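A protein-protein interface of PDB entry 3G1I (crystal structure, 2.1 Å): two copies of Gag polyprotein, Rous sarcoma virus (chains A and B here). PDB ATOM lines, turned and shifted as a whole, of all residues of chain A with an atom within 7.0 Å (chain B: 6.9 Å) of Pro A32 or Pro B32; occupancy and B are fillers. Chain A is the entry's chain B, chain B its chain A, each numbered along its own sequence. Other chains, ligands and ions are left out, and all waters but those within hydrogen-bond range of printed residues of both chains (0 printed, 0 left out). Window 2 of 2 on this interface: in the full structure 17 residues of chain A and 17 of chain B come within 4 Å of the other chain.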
ATOM      1  N   VAL A  26       7.079  12.846   5.045  1.00  0.00           N
ATOM      2  CA  VAL A  26       5.943  12.036   5.476  1.00  0.00           C
ATOM      3  C   VAL A  26       5.756  12.125   7.009  1.00  0.00           C
ATOM      4  O   VAL A  26       4.638  12.321   7.495  1.00  0.00           O
ATOM      5  CB  VAL A  26       6.101  10.566   5.006  1.00  0.00           C
ATOM      6  CG1 VAL A  26       5.172   9.615   5.787  1.00  0.00           C
ATOM      7  CG2 VAL A  26       5.867  10.470   3.491  1.00  0.00           C
ATOM      8  N   SER A  29       4.226  15.346   7.849  1.00  0.00           N
ATOM      9  CA  SER A  29       2.940  15.620   7.204  1.00  0.00           C
ATOM     10  C   SER A  29       1.779  15.413   8.175  1.00  0.00           C
ATOM     11  O   SER A  29       1.973  14.971   9.305  1.00  0.00           O
ATOM     12  CB  SER A  29       2.731  14.684   6.008  1.00  0.00           C
ATOM     13  OG  SER A  29       2.579  13.352   6.483  1.00  0.00           O
ATOM     14  N   ASP A  30       0.571  15.680   7.693  1.00  0.00           N
ATOM     15  CA  ASP A  30      -0.652  15.461   8.459  1.00  0.00           C
ATOM     16  C   ASP A  30      -1.197  14.034   8.302  1.00  0.00           C
ATOM     17  O   ASP A  30      -2.405  13.841   8.174  1.00  0.00           O
ATOM     18  CB  ASP A  30      -1.727  16.472   8.032  1.00  0.00           C
ATOM     19  CG  ASP A  30      -2.837  16.622   9.073  1.00  0.00           C
ATOM     20  OD1 ASP A  30      -2.559  16.410  10.259  1.00  0.00           O
ATOM     21  OD2 ASP A  30      -3.980  16.925   8.695  1.00  0.00           O
ATOM     22  N   LEU A  31      -0.311  13.046   8.284  1.00  0.00           N
ATOM     23  CA  LEU A  31      -0.706  11.627   8.153  1.00  0.00           C
ATOM     24  C   LEU A  31      -0.675  10.993   9.528  1.00  0.00           C
ATOM     25  O   LEU A  31       0.248  11.271  10.286  1.00  0.00           O
ATOM     26  CB  LEU A  31       0.286  10.855   7.241  1.00  0.00           C
ATOM     27  CG  LEU A  31       0.147  11.037   5.715  1.00  0.00           C
ATOM     28  CD1 LEU A  31       1.323  10.430   4.974  1.00  0.00           C
ATOM     29  CD2 LEU A  31      -1.178  10.525   5.160  1.00  0.00           C
ATOM     30  N   PRO A  32      -1.655  10.103   9.847  1.00  0.00           N
ATOM     31  CA  PRO A  32      -1.492   9.308  11.072  1.00  0.00           C
ATOM     32  C   PRO A  32      -0.278   8.402  10.966  1.00  0.00           C
ATOM     33  O   PRO A  32       0.092   8.001   9.856  1.00  0.00           O
ATOM     34  CB  PRO A  32      -2.758   8.465  11.117  1.00  0.00           C
ATOM     35  CG  PRO A  32      -3.151   8.337   9.680  1.00  0.00           C
ATOM     36  CD  PRO A  32      -2.857   9.695   9.108  1.00  0.00           C
ATOM     37  N   PRO A  33       0.354   8.087  12.105  1.00  0.00           N
ATOM     38  CA  PRO A  33       1.489   7.168  12.096  1.00  0.00           C
ATOM     39  C   PRO A  33       1.191   5.841  11.344  1.00  0.00           C
ATOM     40  O   PRO A  33       2.068   5.313  10.648  1.00  0.00           O
ATOM     41  CB  PRO A  33       1.732   6.919  13.584  1.00  0.00           C
ATOM     42  CG  PRO A  33       1.359   8.228  14.232  1.00  0.00           C
ATOM     43  CD  PRO A  33       0.195   8.761  13.413  1.00  0.00           C
ATOM     44  N   SER A  34      -0.032   5.326  11.479  1.00  0.00           N
ATOM     45  CA  SER A  34      -0.435   4.084  10.800  1.00  0.00           C
ATOM     46  C   SER A  34      -0.416   4.167   9.263  1.00  0.00           C
ATOM     47  O   SER A  34      -0.497   3.150   8.579  1.00  0.00           O
ATOM     48  CB  SER A  34      -1.813   3.634  11.285  1.00  0.00           C
ATOM     49  OG  SER A  34      -2.835   4.519  10.862  1.00  0.00           O
ATOM     50  N   ALA A  35      -0.316   5.371   8.715  1.00  0.00           N
ATOM     51  CA  ALA A  35      -0.348   5.531   7.272  1.00  0.00           C
ATOM     52  C   ALA A  35       1.053   5.793   6.713  1.00  0.00           C
ATOM     53  O   ALA A  35       1.247   5.789   5.487  1.00  0.00           O
ATOM     54  CB  ALA A  35      -1.309   6.637   6.872  1.00  0.00           C
ATOM     55  N   ARG A  36       2.016   6.010   7.610  1.00  0.00           N
ATOM     56  CA  ARG A  36       3.333   6.482   7.203  1.00  0.00           C
ATOM     57  C   ARG A  36       4.120   5.438   6.434  1.00  0.00           C
ATOM     58  O   ARG A  36       4.577   5.728   5.351  1.00  0.00           O
ATOM     59  CB  ARG A  36       4.128   7.051   8.382  1.00  0.00           C
ATOM     60  CG  ARG A  36       3.407   8.286   8.943  1.00  0.00           C
ATOM     61  CD  ARG A  36       4.180   8.958  10.055  1.00  0.00           C
ATOM     62  NE  ARG A  36       3.357  10.031  10.619  1.00  0.00           N
ATOM     63  CZ  ARG A  36       3.504  10.508  11.845  1.00  0.00           C
ATOM     64  NH1 ARG A  36       4.452  10.009  12.624  1.00  0.00           N
ATOM     65  NH2 ARG A  36       2.706  11.489  12.282  1.00  0.00           N
ATOM     66  N   ALA A  37       4.287   4.244   6.987  1.00  0.00           N
ATOM     67  CA  ALA A  37       5.009   3.190   6.256  1.00  0.00           C
ATOM     68  C   ALA A  37       4.344   2.863   4.896  1.00  0.00           C
ATOM     69  O   ALA A  37       5.038   2.829   3.881  1.00  0.00           O
ATOM     70  CB  ALA A  37       5.186   1.929   7.133  1.00  0.00           C
ATOM     71  N   VAL B  26     -11.371   0.130   5.238  1.00  0.00           N
ATOM     72  CA  VAL B  26     -10.492   1.267   5.097  1.00  0.00           C
ATOM     73  C   VAL B  26     -11.283   2.544   4.746  1.00  0.00           C
ATOM     74  O   VAL B  26     -11.013   3.628   5.294  1.00  0.00           O
ATOM     75  CB  VAL B  26      -9.346   0.999   4.099  1.00  0.00           C
ATOM     76  CG1 VAL B  26      -8.692   2.302   3.692  1.00  0.00           C
ATOM     77  CG2 VAL B  26      -8.311   0.043   4.719  1.00  0.00           C
ATOM     78  N   SER B  29     -12.958   3.959   7.716  1.00  0.00           N
ATOM     79  CA  SER B  29     -12.052   4.215   8.834  1.00  0.00           C
ATOM     80  C   SER B  29     -11.826   5.709   9.091  1.00  0.00           C
ATOM     81  O   SER B  29     -12.424   6.579   8.429  1.00  0.00           O
ATOM     82  CB  SER B  29     -10.706   3.495   8.645  1.00  0.00           C
ATOM     83  OG  SER B  29      -9.862   4.239   7.768  1.00  0.00           O
ATOM     84  N   ASP B  30     -10.946   5.996  10.041  1.00  0.00           N
ATOM     85  CA  ASP B  30     -10.554   7.389  10.356  1.00  0.00           C
ATOM     86  C   ASP B  30      -9.401   7.914   9.495  1.00  0.00           C
ATOM     87  O   ASP B  30      -8.972   9.040   9.691  1.00  0.00           O
ATOM     88  CB  ASP B  30     -10.202   7.537  11.860  1.00  0.00           C
ATOM     89  CG  ASP B  30     -11.398   7.192  12.766  1.00  0.00           C
ATOM     90  OD1 ASP B  30     -12.552   7.449  12.346  1.00  0.00           O
ATOM     91  OD2 ASP B  30     -11.180   6.629  13.861  1.00  0.00           O
ATOM     92  N   LEU B  31      -8.893   7.118   8.544  1.00  0.00           N
ATOM     93  CA  LEU B  31      -7.769   7.590   7.721  1.00  0.00           C
ATOM     94  C   LEU B  31      -8.189   8.785   6.874  1.00  0.00           C
ATOM     95  O   LEU B  31      -9.316   8.857   6.439  1.00  0.00           O
ATOM     96  CB  LEU B  31      -7.195   6.472   6.817  1.00  0.00           C
ATOM     97  CG  LEU B  31      -6.471   5.323   7.528  1.00  0.00           C
ATOM     98  CD1 LEU B  31      -6.437   4.036   6.673  1.00  0.00           C
ATOM     99  CD2 LEU B  31      -5.066   5.739   7.885  1.00  0.00           C
ATOM    100  N   PRO B  32      -7.288   9.743   6.645  1.00  0.00           N
ATOM    101  CA  PRO B  32      -7.645  10.755   5.645  1.00  0.00           C
ATOM    102  C   PRO B  32      -7.829  10.072   4.275  1.00  0.00           C
ATOM    103  O   PRO B  32      -7.107   9.113   4.000  1.00  0.00           O
ATOM    104  CB  PRO B  32      -6.431  11.684   5.632  1.00  0.00           C
ATOM    105  CG  PRO B  32      -5.332  10.936   6.238  1.00  0.00           C
ATOM    106  CD  PRO B  32      -5.922   9.888   7.143  1.00  0.00           C
ATOM    107  N   PRO B  33      -8.791  10.529   3.447  1.00  0.00           N
ATOM    108  CA  PRO B  33      -9.001   9.848   2.158  1.00  0.00           C
ATOM    109  C   PRO B  33      -7.738   9.607   1.327  1.00  0.00           C
ATOM    110  O   PRO B  33      -7.663   8.578   0.635  1.00  0.00           O
ATOM    111  CB  PRO B  33      -9.973  10.766   1.424  1.00  0.00           C
ATOM    112  CG  PRO B  33     -10.816  11.378   2.597  1.00  0.00           C
ATOM    113  CD  PRO B  33      -9.815  11.576   3.695  1.00  0.00           C
ATOM    114  N   SER B  34      -6.755  10.501   1.433  1.00  0.00           N
ATOM    115  CA  SER B  34      -5.534  10.412   0.634  1.00  0.00           C
ATOM    116  C   SER B  34      -4.634   9.259   1.070  1.00  0.00           C
ATOM    117  O   SER B  34      -3.719   8.880   0.338  1.00  0.00           O
ATOM    118  CB  SER B  34      -4.735  11.722   0.697  1.00  0.00           C
ATOM    119  OG  SER B  34      -3.998  11.773   1.929  1.00  0.00           O
ATOM    120  N   ALA B  35      -4.874   8.711   2.262  1.00  0.00           N
ATOM    121  CA  ALA B  35      -4.039   7.631   2.747  1.00  0.00           C
ATOM    122  C   ALA B  35      -4.636   6.252   2.411  1.00  0.00           C
ATOM    123  O   ALA B  35      -3.985   5.253   2.591  1.00  0.00           O
ATOM    124  CB  ALA B  35      -3.806   7.760   4.257  1.00  0.00           C
ATOM    125  N   ARG B  36      -5.882   6.225   1.960  1.00  0.00           N
ATOM    126  CA  ARG B  36      -6.620   4.985   1.804  1.00  0.00           C
ATOM    127  C   ARG B  36      -5.993   4.074   0.740  1.00  0.00           C
ATOM    128  O   ARG B  36      -5.810   2.890   0.984  1.00  0.00           O
ATOM    129  CB  ARG B  36      -8.082   5.277   1.430  1.00  0.00           C
ATOM    130  CG  ARG B  36      -8.908   5.880   2.548  1.00  0.00           C
ATOM    131  CD  ARG B  36     -10.310   6.166   2.039  1.00  0.00           C
ATOM    132  NE  ARG B  36     -11.121   6.875   3.030  1.00  0.00           N
ATOM    133  CZ  ARG B  36     -12.165   7.645   2.741  1.00  0.00           C
ATOM    134  NH1 ARG B  36     -12.553   7.826   1.479  1.00  0.00           N
ATOM    135  NH2 ARG B  36     -12.820   8.254   3.715  1.00  0.00           N
ATOM    136  N   ALA B  37      -5.653   4.639  -0.425  1.00  0.00           N
ATOM    137  CA  ALA B  37      -5.175   3.795  -1.548  1.00  0.00           C
ATOM    138  C   ALA B  37      -3.833   3.131  -1.176  1.00  0.00           C
ATOM    139  O   ALA B  37      -3.724   1.918  -1.233  1.00  0.00           O
ATOM    140  CB  ALA B  37      -5.067   4.618  -2.838  1.00  0.00           C
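Pro A32 touches Leu B31, but with the chains exchanged Leu A31 does not touch Pro B32 (4.3 Å). Pro B32 touches its own counterpart, Pro A32. Ser A34 touches Leu B31, but with the chains exchanged Leu A31 does not touch Ser B34 (4.5 Å). Ala B35 touches its own counterpart, Ala A35. Of the 6 pairs that touch across the chains among the printed residues, 4 have their exchanged pair printed and touching as well.
Among the printed residues, merely in contact across the chains: Pro A32 with Pro B32, Pro A32 with Leu B31, Ala A35 with Ala B35, Ser A34 with Leu B31, Leu A31 with Ala B35 and Ala A35 with Leu B31.
Printed residues of chain B that touch a printed residue of chain A: Leu B31, Pro B32 and Ala B35. Among the printed residues, 6 pairs touch across the chains.
N of Leu A31 sits close to OG of Ser A29 (3.4 Å). OG of Ser B29 lies within hydrogen-bond range of N of Leu B31 (3.1 Å). The guanidinium group (NH2) of Arg A36 lies within hydrogen-bond range of the backbone carbonyl oxygen (O) of Leu A31, 3.2 Å away.
Of the printed residues of chain B, Leu A31 touches Ala B35 (3.9 Å). Pro A32 touches two residues of chain B. Of the printed residues of chain B, Ser A34 touches Leu B31. Ala A37 touches none of the printed residues of chain B. Pro B32 touches just one residue of chain A: Pro A32. Of the printed residues of chain A, Ala B35 touches Leu A31 and Ala A35. The nearest residue of chain B that does not touch Pro A32 is Ala B35 (5.3 Å). The nearest residue of chain A that does not touch Pro B32 is Leu A31 (4.3 Å).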
